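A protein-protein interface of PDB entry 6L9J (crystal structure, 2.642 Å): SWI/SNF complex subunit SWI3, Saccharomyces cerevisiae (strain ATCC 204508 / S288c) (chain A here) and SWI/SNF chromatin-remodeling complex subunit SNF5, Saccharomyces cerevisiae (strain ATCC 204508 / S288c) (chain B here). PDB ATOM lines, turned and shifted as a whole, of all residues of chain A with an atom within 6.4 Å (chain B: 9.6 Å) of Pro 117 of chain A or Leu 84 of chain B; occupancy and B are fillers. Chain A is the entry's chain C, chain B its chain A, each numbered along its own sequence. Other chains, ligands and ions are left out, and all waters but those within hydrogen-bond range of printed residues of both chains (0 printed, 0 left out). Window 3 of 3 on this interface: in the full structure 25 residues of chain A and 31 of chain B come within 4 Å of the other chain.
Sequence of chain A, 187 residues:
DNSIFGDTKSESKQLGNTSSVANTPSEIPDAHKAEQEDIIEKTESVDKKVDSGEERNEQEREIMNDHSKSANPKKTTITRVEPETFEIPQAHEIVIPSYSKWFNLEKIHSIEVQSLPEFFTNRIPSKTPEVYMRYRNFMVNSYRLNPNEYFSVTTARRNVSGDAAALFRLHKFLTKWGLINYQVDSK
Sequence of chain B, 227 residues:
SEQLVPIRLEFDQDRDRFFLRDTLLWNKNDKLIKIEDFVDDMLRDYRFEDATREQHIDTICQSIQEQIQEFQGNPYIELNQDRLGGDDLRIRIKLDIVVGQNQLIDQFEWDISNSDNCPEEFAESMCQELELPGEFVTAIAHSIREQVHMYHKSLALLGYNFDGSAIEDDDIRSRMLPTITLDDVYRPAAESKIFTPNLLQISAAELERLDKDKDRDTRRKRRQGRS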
ATOM      1  N   GLU A 112      15.913  13.321 -16.224  1.00  0.00           N
ATOM      2  CA  GLU A 112      17.001  14.224 -16.583  1.00  0.00           C
ATOM      3  C   GLU A 112      16.684  14.989 -17.856  1.00  0.00           C
ATOM      4  O   GLU A 112      17.104  16.139 -18.013  1.00  0.00           O
ATOM      5  CB  GLU A 112      18.309  13.458 -16.766  1.00  0.00           C
ATOM      6  CG  GLU A 112      18.751  12.623 -15.591  1.00  0.00           C
ATOM      7  CD  GLU A 112      20.011  11.854 -15.901  1.00  0.00           C
ATOM      8  OE1 GLU A 112      21.102  12.422 -15.699  1.00  0.00           O
ATOM      9  OE2 GLU A 112      19.917  10.701 -16.374  1.00  0.00           O
ATOM     10  N   VAL A 113      15.978  14.364 -18.797  1.00  0.00           N
ATOM     11  CA  VAL A 113      15.651  15.087 -20.014  1.00  0.00           C
ATOM     12  C   VAL A 113      14.554  16.098 -19.769  1.00  0.00           C
ATOM     13  O   VAL A 113      14.414  17.048 -20.540  1.00  0.00           O
ATOM     14  CB  VAL A 113      15.250  14.132 -21.141  1.00  0.00           C
ATOM     15  CG1 VAL A 113      15.107  14.901 -22.438  1.00  0.00           C
ATOM     16  CG2 VAL A 113      16.279  13.046 -21.268  1.00  0.00           C
ATOM     17  N   GLN A 114      13.779  15.928 -18.704  1.00  0.00           N
ATOM     18  CA  GLN A 114      12.772  16.918 -18.355  1.00  0.00           C
ATOM     19  C   GLN A 114      13.330  18.038 -17.490  1.00  0.00           C
ATOM     20  O   GLN A 114      12.959  19.198 -17.686  1.00  0.00           O
ATOM     21  CB  GLN A 114      11.606  16.252 -17.626  1.00  0.00           C
ATOM     22  CG  GLN A 114      10.773  15.325 -18.472  1.00  0.00           C
ATOM     23  CD  GLN A 114       9.820  14.514 -17.628  1.00  0.00           C
ATOM     24  OE1 GLN A 114       9.413  14.943 -16.544  1.00  0.00           O
ATOM     25  NE2 GLN A 114       9.466  13.326 -18.111  1.00  0.00           N
ATOM     26  N   SER A 115      14.213  17.708 -16.532  1.00  0.00           N
ATOM     27  CA  SER A 115      14.794  18.700 -15.629  1.00  0.00           C
ATOM     28  C   SER A 115      15.853  19.569 -16.304  1.00  0.00           C
ATOM     29  O   SER A 115      15.993  20.738 -15.953  1.00  0.00           O
ATOM     30  CB  SER A 115      15.407  18.017 -14.409  1.00  0.00           C
ATOM     31  OG  SER A 115      14.463  17.673 -13.417  1.00  0.00           O
ATOM     32  N   LEU A 116      16.609  19.045 -17.258  1.00  0.00           N
ATOM     33  CA  LEU A 116      17.724  19.779 -17.854  1.00  0.00           C
ATOM     34  C   LEU A 116      17.532  19.869 -19.358  1.00  0.00           C
ATOM     35  O   LEU A 116      18.387  19.448 -20.139  1.00  0.00           O
ATOM     36  CB  LEU A 116      19.071  19.147 -17.510  1.00  0.00           C
ATOM     37  CG  LEU A 116      19.467  19.183 -16.037  1.00  0.00           C
ATOM     38  CD1 LEU A 116      20.703  18.363 -15.801  1.00  0.00           C
ATOM     39  CD2 LEU A 116      19.673  20.595 -15.584  1.00  0.00           C
ATOM     40  N   PRO A 117      16.456  20.446 -19.781  1.00  0.00           N
ATOM     41  CA  PRO A 117      16.126  20.484 -21.207  1.00  0.00           C
ATOM     42  C   PRO A 117      17.072  21.246 -22.115  1.00  0.00           C
ATOM     43  O   PRO A 117      16.713  21.462 -23.272  1.00  0.00           O
ATOM     44  CB  PRO A 117      14.762  21.170 -21.211  1.00  0.00           C
ATOM     45  CG  PRO A 117      14.737  21.934 -19.961  1.00  0.00           C
ATOM     46  CD  PRO A 117      15.434  21.095 -18.962  1.00  0.00           C
ATOM     47  N   GLU A 118      18.243  21.683 -21.663  1.00  0.00           N
ATOM     48  CA  GLU A 118      19.091  22.432 -22.584  1.00  0.00           C
ATOM     49  C   GLU A 118      20.038  21.545 -23.381  1.00  0.00           C
ATOM     50  O   GLU A 118      20.497  21.961 -24.449  1.00  0.00           O
ATOM     51  CB  GLU A 118      19.884  23.518 -21.843  1.00  0.00           C
ATOM     52  CG  GLU A 118      20.795  23.008 -20.745  1.00  0.00           C
ATOM     53  CD  GLU A 118      21.404  24.121 -19.923  1.00  0.00           C
ATOM     54  OE1 GLU A 118      22.149  24.950 -20.493  1.00  0.00           O
ATOM     55  OE2 GLU A 118      21.132  24.160 -18.706  1.00  0.00           O
ATOM     56  N   PHE A 119      20.317  20.332 -22.918  1.00  0.00           N
ATOM     57  CA  PHE A 119      21.161  19.402 -23.659  1.00  0.00           C
ATOM     58  C   PHE A 119      20.382  18.512 -24.624  1.00  0.00           C
ATOM     59  O   PHE A 119      20.988  17.706 -25.333  1.00  0.00           O
ATOM     60  CB  PHE A 119      21.957  18.539 -22.677  1.00  0.00           C
ATOM     61  CG  PHE A 119      22.812  19.340 -21.748  1.00  0.00           C
ATOM     62  CD1 PHE A 119      24.057  19.789 -22.146  1.00  0.00           C
ATOM     63  CD2 PHE A 119      22.355  19.685 -20.490  1.00  0.00           C
ATOM     64  CE1 PHE A 119      24.822  20.549 -21.306  1.00  0.00           C
ATOM     65  CE2 PHE A 119      23.133  20.447 -19.647  1.00  0.00           C
ATOM     66  CZ  PHE A 119      24.362  20.876 -20.060  1.00  0.00           C
ATOM     67  N   PHE A 120      19.065  18.657 -24.701  1.00  0.00           N
ATOM     68  CA  PHE A 120      18.238  17.689 -25.397  1.00  0.00           C
ATOM     69  C   PHE A 120      17.458  18.253 -26.573  1.00  0.00           C
ATOM     70  O   PHE A 120      16.998  17.475 -27.402  1.00  0.00           O
ATOM     71  CB  PHE A 120      17.309  17.021 -24.389  1.00  0.00           C
ATOM     72  CG  PHE A 120      18.061  16.406 -23.250  1.00  0.00           C
ATOM     73  CD1 PHE A 120      19.162  15.610 -23.497  1.00  0.00           C
ATOM     74  CD2 PHE A 120      17.719  16.656 -21.940  1.00  0.00           C
ATOM     75  CE1 PHE A 120      19.872  15.040 -22.468  1.00  0.00           C
ATOM     76  CE2 PHE A 120      18.444  16.084 -20.901  1.00  0.00           C
ATOM     77  CZ  PHE A 120      19.514  15.272 -21.174  1.00  0.00           C
ATOM     78  N   THR A 121      17.337  19.567 -26.706  1.00  0.00           N
ATOM     79  CA  THR A 121      17.130  20.136 -28.029  1.00  0.00           C
ATOM     80  C   THR A 121      18.140  19.512 -28.974  1.00  0.00           C
ATOM     81  O   THR A 121      19.154  18.977 -28.519  1.00  0.00           O
ATOM     82  CB  THR A 121      17.317  21.653 -28.019  1.00  0.00           C
ATOM     83  OG1 THR A 121      17.580  22.096 -29.357  1.00  0.00           O
ATOM     84  CG2 THR A 121      18.486  22.044 -27.143  1.00  0.00           C
ATOM     85  N   ARG A 123      19.625  21.480 -31.377  1.00  0.00           N
ATOM     86  CA  ARG A 123      19.920  22.718 -32.071  1.00  0.00           C
ATOM     87  C   ARG A 123      21.203  23.402 -31.611  1.00  0.00           C
ATOM     88  O   ARG A 123      21.639  24.355 -32.263  1.00  0.00           O
ATOM     89  CB  ARG A 123      18.740  23.682 -31.904  1.00  0.00           C
ATOM     90  CG  ARG A 123      18.778  24.907 -32.773  1.00  0.00           C
ATOM     91  CD  ARG A 123      17.686  25.844 -32.323  1.00  0.00           C
ATOM     92  NE  ARG A 123      17.705  25.941 -30.870  1.00  0.00           N
ATOM     93  CZ  ARG A 123      18.473  26.789 -30.198  1.00  0.00           C
ATOM     94  NH1 ARG A 123      19.269  27.621 -30.854  1.00  0.00           N
ATOM     95  NH2 ARG A 123      18.437  26.810 -28.875  1.00  0.00           N
ATOM     96  N   ILE A 124      21.810  22.953 -30.522  1.00  0.00           N
ATOM     97  CA  ILE A 124      23.051  23.506 -30.001  1.00  0.00           C
ATOM     98  C   ILE A 124      24.121  22.426 -30.084  1.00  0.00           C
ATOM     99  O   ILE A 124      24.171  21.524 -29.248  1.00  0.00           O
ATOM    100  CB  ILE A 124      22.886  23.996 -28.551  1.00  0.00           C
ATOM    101  CG1 ILE A 124      21.581  24.765 -28.371  1.00  0.00           C
ATOM    102  CG2 ILE A 124      24.080  24.847 -28.140  1.00  0.00           C
ATOM    103  CD1 ILE A 124      21.086  24.759 -26.956  1.00  0.00           C
ATOM    104  N   TYR B  76      18.176  39.457 -26.533  1.00  0.00           N
ATOM    105  CA  TYR B  76      17.318  38.288 -26.676  1.00  0.00           C
ATOM    106  C   TYR B  76      15.953  38.542 -26.052  1.00  0.00           C
ATOM    107  O   TYR B  76      14.919  38.354 -26.697  1.00  0.00           O
ATOM    108  CB  TYR B  76      18.006  37.062 -26.069  1.00  0.00           C
ATOM    109  CG  TYR B  76      19.168  36.612 -26.921  1.00  0.00           C
ATOM    110  CD1 TYR B  76      19.034  35.558 -27.801  1.00  0.00           C
ATOM    111  CD2 TYR B  76      20.388  37.280 -26.882  1.00  0.00           C
ATOM    112  CE1 TYR B  76      20.079  35.163 -28.600  1.00  0.00           C
ATOM    113  CE2 TYR B  76      21.440  36.892 -27.680  1.00  0.00           C
ATOM    114  CZ  TYR B  76      21.279  35.830 -28.538  1.00  0.00           C
ATOM    115  OH  TYR B  76      22.311  35.419 -29.346  1.00  0.00           O
ATOM    116  N   GLN B  81      13.002  35.762 -29.281  1.00  0.00           N
ATOM    117  CA  GLN B  81      13.519  34.456 -29.687  1.00  0.00           C
ATOM    118  C   GLN B  81      13.045  33.368 -28.737  1.00  0.00           C
ATOM    119  O   GLN B  81      12.322  32.451 -29.139  1.00  0.00           O
ATOM    120  CB  GLN B  81      15.043  34.432 -29.727  1.00  0.00           C
ATOM    121  CG  GLN B  81      15.663  35.535 -30.505  1.00  0.00           C
ATOM    122  CD  GLN B  81      16.479  36.393 -29.604  1.00  0.00           C
ATOM    123  OE1 GLN B  81      16.304  36.349 -28.390  1.00  0.00           O
ATOM    124  NE2 GLN B  81      17.392  37.165 -30.174  1.00  0.00           N
ATOM    125  N   ASP B  82      13.465  33.447 -27.476  1.00  0.00           N
ATOM    126  CA  ASP B  82      13.053  32.480 -26.466  1.00  0.00           C
ATOM    127  C   ASP B  82      13.389  31.062 -26.919  1.00  0.00           C
ATOM    128  O   ASP B  82      12.555  30.155 -26.881  1.00  0.00           O
ATOM    129  CB  ASP B  82      11.561  32.622 -26.153  1.00  0.00           C
ATOM    130  CG  ASP B  82      11.156  31.911 -24.874  1.00  0.00           C
ATOM    131  OD1 ASP B  82      11.884  31.004 -24.424  1.00  0.00           O
ATOM    132  OD2 ASP B  82      10.097  32.261 -24.315  1.00  0.00           O
ATOM    133  N   ARG B  83      14.624  30.880 -27.382  1.00  0.00           N
ATOM    134  CA  ARG B  83      15.145  29.553 -27.692  1.00  0.00           C
ATOM    135  C   ARG B  83      15.795  28.996 -26.436  1.00  0.00           C
ATOM    136  O   ARG B  83      16.797  29.533 -25.960  1.00  0.00           O
ATOM    137  CB  ARG B  83      16.140  29.614 -28.843  1.00  0.00           C
ATOM    138  CG  ARG B  83      15.509  29.978 -30.151  1.00  0.00           C
ATOM    139  CD  ARG B  83      16.527  29.941 -31.252  1.00  0.00           C
ATOM    140  NE  ARG B  83      17.609  30.882 -31.009  1.00  0.00           N
ATOM    141  CZ  ARG B  83      17.521  32.184 -31.237  1.00  0.00           C
ATOM    142  NH1 ARG B  83      16.396  32.702 -31.711  1.00  0.00           N
ATOM    143  NH2 ARG B  83      18.558  32.971 -30.997  1.00  0.00           N
ATOM    144  N   LEU B  84      15.225  27.926 -25.894  1.00  0.00           N
ATOM    145  CA  LEU B  84      15.728  27.376 -24.646  1.00  0.00           C
ATOM    146  C   LEU B  84      17.154  26.871 -24.817  1.00  0.00           C
ATOM    147  O   LEU B  84      17.467  26.168 -25.782  1.00  0.00           O
ATOM    148  CB  LEU B  84      14.812  26.252 -24.170  1.00  0.00           C
ATOM    149  CG  LEU B  84      15.147  25.613 -22.825  1.00  0.00           C
ATOM    150  CD1 LEU B  84      15.688  26.645 -21.839  1.00  0.00           C
ATOM    151  CD2 LEU B  84      13.916  24.917 -22.271  1.00  0.00           C
ATOM    152  N   GLY B  85      18.025  27.246 -23.883  1.00  0.00           N
ATOM    153  CA  GLY B  85      19.403  26.809 -23.895  1.00  0.00           C
ATOM    154  C   GLY B  85      20.330  27.612 -24.773  1.00  0.00           C
ATOM    155  O   GLY B  85      21.509  27.262 -24.875  1.00  0.00           O
ATOM    156  N   GLY B  86      19.839  28.659 -25.425  1.00  0.00           N
ATOM    157  CA  GLY B  86      20.684  29.579 -26.163  1.00  0.00           C
ATOM    158  C   GLY B  86      21.317  29.041 -27.429  1.00  0.00           C
ATOM    159  O   GLY B  86      21.206  27.854 -27.733  1.00  0.00           O
ATOM    160  N   ASP B  87      21.999  29.915 -28.170  1.00  0.00           N
ATOM    161  CA  ASP B  87      22.664  29.566 -29.420  1.00  0.00           C
ATOM    162  C   ASP B  87      24.162  29.341 -29.235  1.00  0.00           C
ATOM    163  O   ASP B  87      24.937  29.518 -30.182  1.00  0.00           O
ATOM    164  CB  ASP B  87      22.428  30.649 -30.472  1.00  0.00           C
ATOM    165  CG  ASP B  87      21.265  31.563 -30.131  1.00  0.00           C
ATOM    166  OD1 ASP B  87      20.279  31.097 -29.525  1.00  0.00           O
ATOM    167  OD2 ASP B  87      21.345  32.760 -30.473  1.00  0.00           O
ATOM    168  N   ASP B  88      24.577  28.966 -28.028  1.00  0.00           N
ATOM    169  CA  ASP B  88      25.961  28.633 -27.696  1.00  0.00           C
ATOM    170  C   ASP B  88      26.953  29.704 -28.150  1.00  0.00           C
ATOM    171  O   ASP B  88      27.860  29.446 -28.934  1.00  0.00           O
ATOM    172  CB  ASP B  88      26.345  27.281 -28.284  1.00  0.00           C
ATOM    173  CG  ASP B  88      27.730  26.854 -27.874  1.00  0.00           C
ATOM    174  OD1 ASP B  88      28.514  26.456 -28.759  1.00  0.00           O
ATOM    175  OD2 ASP B  88      28.025  26.916 -26.664  1.00  0.00           O
ATOM    176  N   ASP B 111      27.718  31.912 -21.278  1.00  0.00           N
ATOM    177  CA  ASP B 111      26.916  31.969 -22.494  1.00  0.00           C
ATOM    178  C   ASP B 111      26.116  33.265 -22.508  1.00  0.00           C
ATOM    179  O   ASP B 111      25.323  33.521 -21.599  1.00  0.00           O
ATOM    180  CB  ASP B 111      26.003  30.746 -22.553  1.00  0.00           C
ATOM    181  CG  ASP B 111      25.271  30.603 -23.874  1.00  0.00           C
ATOM    182  OD1 ASP B 111      25.581  31.300 -24.852  1.00  0.00           O
ATOM    183  OD2 ASP B 111      24.378  29.747 -23.933  1.00  0.00           O
ATOM    184  N   SER B 113      23.908  34.165 -24.747  1.00  0.00           N
ATOM    185  CA  SER B 113      22.666  34.001 -25.485  1.00  0.00           C
ATOM    186  C   SER B 113      21.740  33.009 -24.805  1.00  0.00           C
ATOM    187  O   SER B 113      20.983  32.309 -25.469  1.00  0.00           O
ATOM    188  CB  SER B 113      22.946  33.549 -26.913  1.00  0.00           C
ATOM    189  OG  SER B 113      23.333  32.189 -26.932  1.00  0.00           O
ATOM    190  N   ASN B 114      21.811  32.912 -23.485  1.00  0.00           N
ATOM    191  CA  ASN B 114      20.884  32.100 -22.704  1.00  0.00           C
ATOM    192  C   ASN B 114      20.440  32.982 -21.546  1.00  0.00           C
ATOM    193  O   ASN B 114      21.186  33.172 -20.580  1.00  0.00           O
ATOM    194  CB  ASN B 114      21.518  30.800 -22.216  1.00  0.00           C
ATOM    195  CG  ASN B 114      20.574  29.979 -21.359  1.00  0.00           C
ATOM    196  OD1 ASN B 114      19.689  30.522 -20.708  1.00  0.00           O
ATOM    197  ND2 ASN B 114      20.756  28.670 -21.356  1.00  0.00           N
ATOM    198  N   SER B 115      19.228  33.520 -21.655  1.00  0.00           N
ATOM    199  CA  SER B 115      18.712  34.479 -20.694  1.00  0.00           C
ATOM    200  C   SER B 115      18.265  33.837 -19.393  1.00  0.00           C
ATOM    201  O   SER B 115      17.725  34.531 -18.532  1.00  0.00           O
ATOM    202  CB  SER B 115      17.564  35.270 -21.313  1.00  0.00           C
ATOM    203  OG  SER B 115      16.490  34.414 -21.647  1.00  0.00           O
ATOM    204  N   ASP B 116      18.484  32.546 -19.210  1.00  0.00           N
ATOM    205  CA  ASP B 116      18.257  31.927 -17.915  1.00  0.00           C
ATOM    206  C   ASP B 116      19.532  31.784 -17.093  1.00  0.00           C
ATOM    207  O   ASP B 116      19.476  31.252 -15.983  1.00  0.00           O
ATOM    208  CB  ASP B 116      17.575  30.565 -18.088  1.00  0.00           C
ATOM    209  CG  ASP B 116      16.114  30.695 -18.507  1.00  0.00           C
ATOM    210  OD1 ASP B 116      15.625  29.817 -19.248  1.00  0.00           O
ATOM    211  OD2 ASP B 116      15.454  31.679 -18.099  1.00  0.00           O
ATOM    212  N   ASN B 117      20.673  32.235 -17.614  1.00  0.00           N
ATOM    213  CA  ASN B 117      21.899  32.353 -16.830  1.00  0.00           C
ATOM    214  C   ASN B 117      21.783  33.556 -15.903  1.00  0.00           C
ATOM    215  O   ASN B 117      21.697  34.693 -16.367  1.00  0.00           O
ATOM    216  CB  ASN B 117      23.105  32.519 -17.745  1.00  0.00           C
ATOM    217  CG  ASN B 117      23.405  31.286 -18.561  1.00  0.00           C
ATOM    218  OD1 ASN B 117      22.896  30.197 -18.302  1.00  0.00           O
ATOM    219  ND2 ASN B 117      24.263  31.453 -19.551  1.00  0.00           N
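O of Leu 84 of chain B sits at hydrogen-bond distance from NH2 of Arg 123 of chain A. NH2 of Arg 123 of chain A sits at hydrogen-bond distance from O of Gly 86 of chain B (3.2 Å). NH1 of Arg 123 of chain A is in salt-bridge range of OD1 of Asp 87 of chain B, at 3.9 Å.
OH of Tyr 76 of chain B lies within hydrogen-bond range of OD2 of Asp 87 of chain B, at 3.0 Å. NH2 of Arg 83 of chain B lies within salt-bridge range of OD2 of Asp 87 of chain B, 2.8 Å away. The side-chain hydroxyl (OG) of Ser 113 of chain B sits at hydrogen-bond distance from the backbone NH (N) of Asp 87 of chain B, 2.9 Å away. N of Arg 123 of chain A is in hydrogen-bond range of OG1 of Thr 121 of chain A (2.9 Å).
Among the printed residues, merely in contact across the chains: Pro 117 of chain A with Leu 84 of chain B (3.9 Å), Glu 118 of chain A with Gly 85 of chain B (3.9 Å), Arg 123 of chain A with Arg 83 of chain B (3.6 Å), Ile 124 of chain A with Gly 85 of chain B (3.3 Å), Ile 124 of chain A with Gly 86 of chain B (3.2 Å) and Ile 124 of chain A with Asp 88 of chain B (3.3 Å).
Pro 117 of chain A touches one residue of chain B. Printed residues of chain A within 4 Å of Leu 84 of chain B: Pro 117 and Arg 123. Of the printed residues of chain A, Asp 87 of chain B touches Arg 123. Of the printed residues of chain A, Arg 83 of chain B touches Arg 123. Of the printed residues of chain A, Asp 88 of chain B touches Ile 124 (3.3 Å). Printed residues of chain A within 4 Å of Gly 86 of chain B: Arg 123 (3.2 Å) and Ile 124 (3.2 Å). The nearest printed residue of chain B that does not touch Ile 124 of chain A is Leu 84 of chain B (4.1 Å).
Of the 15 printed residues of chain B, 6 touch a printed residue of chain A. Printed residues of chain B that touch a printed residue of chain A: Arg 83, Leu 84, Gly 85, Gly 86, Asp 87 and Asp 88. Along chain A the printed residues that touch a printed residue of chain B span positions 117 to 124. Among the printed residues, 9 pairs touch across the chains.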
